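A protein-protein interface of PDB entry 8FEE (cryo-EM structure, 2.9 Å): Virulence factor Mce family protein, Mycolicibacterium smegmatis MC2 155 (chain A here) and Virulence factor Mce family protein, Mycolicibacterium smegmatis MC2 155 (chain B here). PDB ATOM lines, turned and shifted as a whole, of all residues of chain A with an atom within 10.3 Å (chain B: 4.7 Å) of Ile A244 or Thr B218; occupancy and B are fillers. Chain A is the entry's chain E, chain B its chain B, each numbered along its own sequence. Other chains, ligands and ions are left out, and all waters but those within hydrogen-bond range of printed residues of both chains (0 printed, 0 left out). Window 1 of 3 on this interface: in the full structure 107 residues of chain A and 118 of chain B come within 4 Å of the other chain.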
ATOM      1  N   LEU A 233     -27.738   1.499 -27.635  1.00  0.00           N
ATOM      2  CA  LEU A 233     -27.936   1.966 -26.263  1.00  0.00           C
ATOM      3  C   LEU A 233     -26.885   1.370 -25.326  1.00  0.00           C
ATOM      4  O   LEU A 233     -26.289   2.077 -24.501  1.00  0.00           O
ATOM      5  CB  LEU A 233     -29.346   1.600 -25.796  1.00  0.00           C
ATOM      6  CG  LEU A 233     -30.161   2.615 -24.990  1.00  0.00           C
ATOM      7  CD1 LEU A 233     -31.452   1.977 -24.506  1.00  0.00           C
ATOM      8  CD2 LEU A 233     -29.369   3.164 -23.818  1.00  0.00           C
ATOM      9  N   VAL A 236     -23.457   2.935 -25.998  1.00  0.00           N
ATOM     10  CA  VAL A 236     -23.385   4.267 -25.399  1.00  0.00           C
ATOM     11  C   VAL A 236     -23.138   4.158 -23.902  1.00  0.00           C
ATOM     12  O   VAL A 236     -22.236   4.803 -23.353  1.00  0.00           O
ATOM     13  CB  VAL A 236     -24.672   5.060 -25.694  1.00  0.00           C
ATOM     14  CG1 VAL A 236     -24.706   6.335 -24.870  1.00  0.00           C
ATOM     15  CG2 VAL A 236     -24.778   5.394 -27.167  1.00  0.00           C
ATOM     16  N   LEU A 237     -23.928   3.321 -23.223  1.00  0.00           N
ATOM     17  CA  LEU A 237     -23.789   3.183 -21.776  1.00  0.00           C
ATOM     18  C   LEU A 237     -22.433   2.609 -21.377  1.00  0.00           C
ATOM     19  O   LEU A 237     -21.923   2.926 -20.296  1.00  0.00           O
ATOM     20  CB  LEU A 237     -24.922   2.318 -21.223  1.00  0.00           C
ATOM     21  CG  LEU A 237     -26.294   2.990 -21.192  1.00  0.00           C
ATOM     22  CD1 LEU A 237     -27.368   2.016 -20.741  1.00  0.00           C
ATOM     23  CD2 LEU A 237     -26.259   4.207 -20.286  1.00  0.00           C
ATOM     24  N   THR A 238     -21.833   1.771 -22.225  1.00  0.00           N
ATOM     25  CA  THR A 238     -20.493   1.269 -21.926  1.00  0.00           C
ATOM     26  C   THR A 238     -19.426   2.340 -22.107  1.00  0.00           C
ATOM     27  O   THR A 238     -18.538   2.485 -21.259  1.00  0.00           O
ATOM     28  CB  THR A 238     -20.157   0.064 -22.808  1.00  0.00           C
ATOM     29  OG1 THR A 238     -20.399   0.389 -24.181  1.00  0.00           O
ATOM     30  CG2 THR A 238     -20.975  -1.149 -22.417  1.00  0.00           C
ATOM     31  N   GLU A 239     -19.494   3.106 -23.196  1.00  0.00           N
ATOM     32  CA  GLU A 239     -18.334   3.890 -23.606  1.00  0.00           C
ATOM     33  C   GLU A 239     -18.393   5.367 -23.238  1.00  0.00           C
ATOM     34  O   GLU A 239     -17.334   5.995 -23.134  1.00  0.00           O
ATOM     35  CB  GLU A 239     -18.110   3.745 -25.114  1.00  0.00           C
ATOM     36  CG  GLU A 239     -18.084   2.293 -25.563  1.00  0.00           C
ATOM     37  CD  GLU A 239     -17.498   2.114 -26.943  1.00  0.00           C
ATOM     38  OE1 GLU A 239     -16.949   3.094 -27.485  1.00  0.00           O
ATOM     39  OE2 GLU A 239     -17.589   0.993 -27.489  1.00  0.00           O
ATOM     40  N   PHE A 240     -19.574   5.947 -23.042  1.00  0.00           N
ATOM     41  CA  PHE A 240     -19.646   7.383 -22.787  1.00  0.00           C
ATOM     42  C   PHE A 240     -19.388   7.816 -21.339  1.00  0.00           C
ATOM     43  O   PHE A 240     -18.762   8.868 -21.150  1.00  0.00           O
ATOM     44  CB  PHE A 240     -20.996   7.928 -23.257  1.00  0.00           C
ATOM     45  CG  PHE A 240     -20.991   8.387 -24.683  1.00  0.00           C
ATOM     46  CD1 PHE A 240     -20.462   9.620 -25.021  1.00  0.00           C
ATOM     47  CD2 PHE A 240     -21.500   7.584 -25.686  1.00  0.00           C
ATOM     48  CE1 PHE A 240     -20.451  10.047 -26.330  1.00  0.00           C
ATOM     49  CE2 PHE A 240     -21.492   8.005 -26.998  1.00  0.00           C
ATOM     50  CZ  PHE A 240     -20.966   9.238 -27.319  1.00  0.00           C
ATOM     51  N   PRO A 241     -19.873   7.114 -20.308  1.00  0.00           N
ATOM     52  CA  PRO A 241     -19.624   7.569 -18.921  1.00  0.00           C
ATOM     53  C   PRO A 241     -18.146   7.745 -18.595  1.00  0.00           C
ATOM     54  O   PRO A 241     -17.799   8.728 -17.921  1.00  0.00           O
ATOM     55  CB  PRO A 241     -20.266   6.466 -18.067  1.00  0.00           C
ATOM     56  CG  PRO A 241     -21.382   5.997 -18.891  1.00  0.00           C
ATOM     57  CD  PRO A 241     -20.896   6.045 -20.317  1.00  0.00           C
ATOM     58  N   PRO A 242     -17.235   6.841 -19.017  1.00  0.00           N
ATOM     59  CA  PRO A 242     -15.810   7.125 -18.756  1.00  0.00           C
ATOM     60  C   PRO A 242     -15.323   8.397 -19.425  1.00  0.00           C
ATOM     61  O   PRO A 242     -14.561   9.165 -18.822  1.00  0.00           O
ATOM     62  CB  PRO A 242     -15.091   5.884 -19.302  1.00  0.00           C
ATOM     63  CG  PRO A 242     -16.104   4.827 -19.301  1.00  0.00           C
ATOM     64  CD  PRO A 242     -17.383   5.507 -19.636  1.00  0.00           C
ATOM     65  N   LEU A 243     -15.753   8.638 -20.666  1.00  0.00           N
ATOM     66  CA  LEU A 243     -15.352   9.845 -21.379  1.00  0.00           C
ATOM     67  C   LEU A 243     -15.854  11.092 -20.665  1.00  0.00           C
ATOM     68  O   LEU A 243     -15.120  12.077 -20.523  1.00  0.00           O
ATOM     69  CB  LEU A 243     -15.872   9.800 -22.815  1.00  0.00           C
ATOM     70  CG  LEU A 243     -15.578  11.023 -23.682  1.00  0.00           C
ATOM     71  CD1 LEU A 243     -14.083  11.264 -23.744  1.00  0.00           C
ATOM     72  CD2 LEU A 243     -16.152  10.842 -25.075  1.00  0.00           C
ATOM     73  N   ILE A 244     -17.110  11.068 -20.213  1.00  0.00           N
ATOM     74  CA  ILE A 244     -17.687  12.232 -19.552  1.00  0.00           C
ATOM     75  C   ILE A 244     -17.014  12.468 -18.205  1.00  0.00           C
ATOM     76  O   ILE A 244     -16.770  13.615 -17.812  1.00  0.00           O
ATOM     77  CB  ILE A 244     -19.211  12.060 -19.414  1.00  0.00           C
ATOM     78  CG1 ILE A 244     -19.851  11.949 -20.798  1.00  0.00           C
ATOM     79  CG2 ILE A 244     -19.820  13.220 -18.650  1.00  0.00           C
ATOM     80  CD1 ILE A 244     -21.352  11.794 -20.768  1.00  0.00           C
ATOM     81  N   GLN A 245     -16.689  11.390 -17.484  1.00  0.00           N
ATOM     82  CA  GLN A 245     -15.944  11.532 -16.236  1.00  0.00           C
ATOM     83  C   GLN A 245     -14.573  12.148 -16.483  1.00  0.00           C
ATOM     84  O   GLN A 245     -14.143  13.046 -15.745  1.00  0.00           O
ATOM     85  CB  GLN A 245     -15.807  10.174 -15.549  1.00  0.00           C
ATOM     86  CG  GLN A 245     -14.904  10.183 -14.328  1.00  0.00           C
ATOM     87  CD  GLN A 245     -14.809   8.823 -13.666  1.00  0.00           C
ATOM     88  OE1 GLN A 245     -15.127   7.802 -14.272  1.00  0.00           O
ATOM     89  NE2 GLN A 245     -14.370   8.806 -12.413  1.00  0.00           N
ATOM     90  N   HIS A 246     -13.877  11.684 -17.526  1.00  0.00           N
ATOM     91  CA  HIS A 246     -12.574  12.251 -17.856  1.00  0.00           C
ATOM     92  C   HIS A 246     -12.691  13.729 -18.195  1.00  0.00           C
ATOM     93  O   HIS A 246     -11.888  14.544 -17.727  1.00  0.00           O
ATOM     94  CB  HIS A 246     -11.943  11.492 -19.022  1.00  0.00           C
ATOM     95  CG  HIS A 246     -10.684  12.121 -19.532  1.00  0.00           C
ATOM     96  ND1 HIS A 246      -9.620  12.427 -18.712  1.00  0.00           N
ATOM     97  CD2 HIS A 246     -10.326  12.515 -20.777  1.00  0.00           C
ATOM     98  CE1 HIS A 246      -8.656  12.976 -19.431  1.00  0.00           C
ATOM     99  NE2 HIS A 246      -9.060  13.039 -20.687  1.00  0.00           N
ATOM    100  N   PHE A 247     -13.696  14.093 -18.999  1.00  0.00           N
ATOM    101  CA  PHE A 247     -13.888  15.493 -19.367  1.00  0.00           C
ATOM    102  C   PHE A 247     -14.175  16.348 -18.141  1.00  0.00           C
ATOM    103  O   PHE A 247     -13.650  17.460 -18.014  1.00  0.00           O
ATOM    104  CB  PHE A 247     -15.019  15.623 -20.386  1.00  0.00           C
ATOM    105  CG  PHE A 247     -14.610  15.297 -21.792  1.00  0.00           C
ATOM    106  CD1 PHE A 247     -13.275  15.290 -22.156  1.00  0.00           C
ATOM    107  CD2 PHE A 247     -15.564  15.015 -22.756  1.00  0.00           C
ATOM    108  CE1 PHE A 247     -12.897  14.997 -23.451  1.00  0.00           C
ATOM    109  CE2 PHE A 247     -15.192  14.723 -24.054  1.00  0.00           C
ATOM    110  CZ  PHE A 247     -13.857  14.716 -24.402  1.00  0.00           C
ATOM    111  N   ALA A 248     -15.016  15.849 -17.231  1.00  0.00           N
ATOM    112  CA  ALA A 248     -15.300  16.580 -16.003  1.00  0.00           C
ATOM    113  C   ALA A 248     -14.053  16.730 -15.144  1.00  0.00           C
ATOM    114  O   ALA A 248     -13.923  17.713 -14.405  1.00  0.00           O
ATOM    115  CB  ALA A 248     -16.407  15.879 -15.217  1.00  0.00           C
ATOM    116  N   GLU A 249     -13.134  15.763 -15.213  1.00  0.00           N
ATOM    117  CA  GLU A 249     -11.865  15.908 -14.505  1.00  0.00           C
ATOM    118  C   GLU A 249     -11.006  17.016 -15.106  1.00  0.00           C
ATOM    119  O   GLU A 249     -10.335  17.752 -14.374  1.00  0.00           O
ATOM    120  CB  GLU A 249     -11.105  14.581 -14.506  1.00  0.00           C
ATOM    121  CG  GLU A 249     -11.735  13.494 -13.649  1.00  0.00           C
ATOM    122  CD  GLU A 249     -11.506  13.706 -12.165  1.00  0.00           C
ATOM    123  OE1 GLU A 249     -10.654  14.546 -11.804  1.00  0.00           O
ATOM    124  OE2 GLU A 249     -12.178  13.031 -11.357  1.00  0.00           O
ATOM    125  N   THR A 250     -11.012  17.156 -16.434  1.00  0.00           N
ATOM    126  CA  THR A 250     -10.122  18.082 -17.128  1.00  0.00           C
ATOM    127  C   THR A 250     -10.864  19.279 -17.720  1.00  0.00           C
ATOM    128  O   THR A 250     -10.400  19.885 -18.690  1.00  0.00           O
ATOM    129  CB  THR A 250      -9.334  17.355 -18.220  1.00  0.00           C
ATOM    130  OG1 THR A 250      -8.449  18.276 -18.866  1.00  0.00           O
ATOM    131  CG2 THR A 250     -10.270  16.763 -19.261  1.00  0.00           C
ATOM    132  N   ARG A 251     -12.015  19.638 -17.142  1.00  0.00           N
ATOM    133  CA  ARG A 251     -12.773  20.781 -17.646  1.00  0.00           C
ATOM    134  C   ARG A 251     -11.988  22.081 -17.499  1.00  0.00           C
ATOM    135  O   ARG A 251     -12.001  22.927 -18.401  1.00  0.00           O
ATOM    136  CB  ARG A 251     -14.118  20.879 -16.927  1.00  0.00           C
ATOM    137  CG  ARG A 251     -14.021  20.798 -15.413  1.00  0.00           C
ATOM    138  CD  ARG A 251     -15.362  21.034 -14.743  1.00  0.00           C
ATOM    139  NE  ARG A 251     -15.328  20.664 -13.333  1.00  0.00           N
ATOM    140  CZ  ARG A 251     -14.858  21.441 -12.366  1.00  0.00           C
ATOM    141  NH1 ARG A 251     -14.383  22.649 -12.619  1.00  0.00           N
ATOM    142  NH2 ARG A 251     -14.865  20.992 -11.114  1.00  0.00           N
ATOM    143  N   GLN B 214     -22.786   3.278 -13.777  1.00  0.00           N
ATOM    144  CA  GLN B 214     -22.269   4.235 -14.750  1.00  0.00           C
ATOM    145  C   GLN B 214     -23.324   5.271 -15.110  1.00  0.00           C
ATOM    146  O   GLN B 214     -23.005   6.451 -15.292  1.00  0.00           O
ATOM    147  CB  GLN B 214     -21.779   3.504 -15.999  1.00  0.00           C
ATOM    148  CG  GLN B 214     -21.017   2.215 -15.717  1.00  0.00           C
ATOM    149  CD  GLN B 214     -19.821   2.415 -14.800  1.00  0.00           C
ATOM    150  OE1 GLN B 214     -19.178   3.465 -14.813  1.00  0.00           O
ATOM    151  NE2 GLN B 214     -19.520   1.403 -13.996  1.00  0.00           N
ATOM    152  N   PHE B 215     -24.581   4.841 -15.239  1.00  0.00           N
ATOM    153  CA  PHE B 215     -25.666   5.761 -15.568  1.00  0.00           C
ATOM    154  C   PHE B 215     -25.877   6.795 -14.470  1.00  0.00           C
ATOM    155  O   PHE B 215     -26.263   7.934 -14.755  1.00  0.00           O
ATOM    156  CB  PHE B 215     -26.952   4.974 -15.830  1.00  0.00           C
ATOM    157  CG  PHE B 215     -28.152   5.837 -16.092  1.00  0.00           C
ATOM    158  CD1 PHE B 215     -28.356   6.401 -17.339  1.00  0.00           C
ATOM    159  CD2 PHE B 215     -29.086   6.068 -15.097  1.00  0.00           C
ATOM    160  CE1 PHE B 215     -29.460   7.192 -17.584  1.00  0.00           C
ATOM    161  CE2 PHE B 215     -30.192   6.858 -15.336  1.00  0.00           C
ATOM    162  CZ  PHE B 215     -30.380   7.419 -16.581  1.00  0.00           C
ATOM    163  N   ASP B 216     -25.653   6.417 -13.212  1.00  0.00           N
ATOM    164  CA  ASP B 216     -25.740   7.379 -12.120  1.00  0.00           C
ATOM    165  C   ASP B 216     -24.514   8.282 -12.058  1.00  0.00           C
ATOM    166  O   ASP B 216     -24.635   9.471 -11.740  1.00  0.00           O
ATOM    167  CB  ASP B 216     -25.924   6.644 -10.792  1.00  0.00           C
ATOM    168  CG  ASP B 216     -25.710   7.544  -9.593  1.00  0.00           C
ATOM    169  OD1 ASP B 216     -26.568   8.413  -9.337  1.00  0.00           O
ATOM    170  OD2 ASP B 216     -24.681   7.382  -8.904  1.00  0.00           O
ATOM    171  N   GLU B 217     -23.329   7.743 -12.353  1.00  0.00           N
ATOM    172  CA  GLU B 217     -22.121   8.564 -12.318  1.00  0.00           C
ATOM    173  C   GLU B 217     -22.102   9.596 -13.440  1.00  0.00           C
ATOM    174  O   GLU B 217     -21.628  10.724 -13.241  1.00  0.00           O
ATOM    175  CB  GLU B 217     -20.878   7.679 -12.390  1.00  0.00           C
ATOM    176  CG  GLU B 217     -20.627   6.847 -11.145  1.00  0.00           C
ATOM    177  CD  GLU B 217     -19.301   6.114 -11.196  1.00  0.00           C
ATOM    178  OE1 GLU B 217     -18.552   6.308 -12.175  1.00  0.00           O
ATOM    179  OE2 GLU B 217     -19.008   5.344 -10.257  1.00  0.00           O
ATOM    180  N   THR B 218     -22.602   9.230 -14.626  1.00  0.00           N
ATOM    181  CA  THR B 218     -22.482  10.119 -15.777  1.00  0.00           C
ATOM    182  C   THR B 218     -23.332  11.373 -15.621  1.00  0.00           C
ATOM    183  O   THR B 218     -22.939  12.433 -16.109  1.00  0.00           O
ATOM    184  CB  THR B 218     -22.837   9.394 -17.080  1.00  0.00           C
ATOM    185  OG1 THR B 218     -22.755  10.317 -18.171  1.00  0.00           O
ATOM    186  CG2 THR B 218     -24.240   8.831 -17.037  1.00  0.00           C
ATOM    187  N   LEU B 219     -24.485  11.281 -14.956  1.00  0.00           N
ATOM    188  CA  LEU B 219     -25.308  12.469 -14.747  1.00  0.00           C
ATOM    189  C   LEU B 219     -24.574  13.499 -13.896  1.00  0.00           C
ATOM    190  O   LEU B 219     -24.525  14.685 -14.241  1.00  0.00           O
ATOM    191  CB  LEU B 219     -26.639  12.082 -14.100  1.00  0.00           C
ATOM    192  CG  LEU B 219     -27.517  11.109 -14.888  1.00  0.00           C
ATOM    193  CD1 LEU B 219     -28.849  10.903 -14.187  1.00  0.00           C
ATOM    194  CD2 LEU B 219     -27.730  11.603 -16.307  1.00  0.00           C
ATOM    195  N   VAL B 220     -23.972  13.055 -12.789  1.00  0.00           N
ATOM    196  CA  VAL B 220     -23.233  13.970 -11.923  1.00  0.00           C
ATOM    197  C   VAL B 220     -21.999  14.511 -12.637  1.00  0.00           C
ATOM    198  O   VAL B 220     -21.677  15.701 -12.526  1.00  0.00           O
ATOM    199  CB  VAL B 220     -22.860  13.269 -10.605  1.00  0.00           C
ATOM    200  CG1 VAL B 220     -22.174  14.244  -9.661  1.00  0.00           C
ATOM    201  CG2 VAL B 220     -24.094  12.670  -9.958  1.00  0.00           C
ATOM    202  N   ASN B 221     -21.284  13.650 -13.368  1.00  0.00           N
ATOM    203  CA  ASN B 221     -20.096  14.110 -14.084  1.00  0.00           C
ATOM    204  C   ASN B 221     -20.458  15.136 -15.150  1.00  0.00           C
ATOM    205  O   ASN B 221     -19.771  16.153 -15.305  1.00  0.00           O
ATOM    206  CB  ASN B 221     -19.359  12.924 -14.705  1.00  0.00           C
ATOM    207  CG  ASN B 221     -18.783  11.987 -13.664  1.00  0.00           C
ATOM    208  OD1 ASN B 221     -18.840  10.767 -13.812  1.00  0.00           O
ATOM    209  ND2 ASN B 221     -18.228  12.555 -12.599  1.00  0.00           N
ATOM    210  N   PHE B 222     -21.536  14.882 -15.894  1.00  0.00           N
ATOM    211  CA  PHE B 222     -21.994  15.817 -16.911  1.00  0.00           C
ATOM    212  C   PHE B 222     -22.423  17.135 -16.286  1.00  0.00           C
ATOM    213  O   PHE B 222     -22.128  18.207 -16.824  1.00  0.00           O
ATOM    214  CB  PHE B 222     -23.143  15.193 -17.702  1.00  0.00           C
ATOM    215  CG  PHE B 222     -23.141  15.541 -19.161  1.00  0.00           C
ATOM    216  CD1 PHE B 222     -22.417  16.621 -19.633  1.00  0.00           C
ATOM    217  CD2 PHE B 222     -23.865  14.781 -20.063  1.00  0.00           C
ATOM    218  CE1 PHE B 222     -22.416  16.938 -20.976  1.00  0.00           C
ATOM    219  CE2 PHE B 222     -23.868  15.092 -21.407  1.00  0.00           C
ATOM    220  CZ  PHE B 222     -23.143  16.172 -21.864  1.00  0.00           C
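The backbone carbonyl oxygen of Glu B217 lies close to the side-chain amide oxygen of Asn B221 (2.8 Å). The guanidinium group (NE) of Arg A251 sits close to the backbone carbonyl oxygen (O) of Ala A248, at 3.4 Å.
Pro A241 touches Gln B214. Ile A244 touches Thr B218 (CD1 to OG1, 3.3 Å). CG2 of Ile A244 touches CB of Asn B221, 3.98 Å away. Phe B222 touches Ile A244 (N to CG2, 3.6 Å). CB of Gln A245 touches OD1 of Asn B221, 3.5 Å away. CB of Ala A248 touches O of Asn B221, at 3.4 Å.
Val A236 touches none of the printed residues of chain B. Printed residues of chain B within 4 Å of Ile A244: Thr B218, Asn B221 and Phe B222. Of the printed residues of chain A, Gln B214 touches Pro A241 (3.8 Å). Printed residues of chain A within 4 Å of Thr B218: Ile A244 (3.3 Å). No residue of chain A comes within 4 Å of Leu B219. Of the printed residues of chain A, Asn B221 touches Ile A244, Gln A245 and Ala A248. Phe B222 touches one residue of chain A. The nearest printed residue of chain B that does not touch Ile A244 is Glu B217 (6.2 Å).
Of the 9 printed residues of chain B, 4 touch a printed residue of chain A. Printed residues of chain B that touch a printed residue of chain A: Gln B214, Thr B218, Asn B221 and Phe B222. Hydrophobic or aromatic side chains of chain B that line the printed part of chain A: Phe B222.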
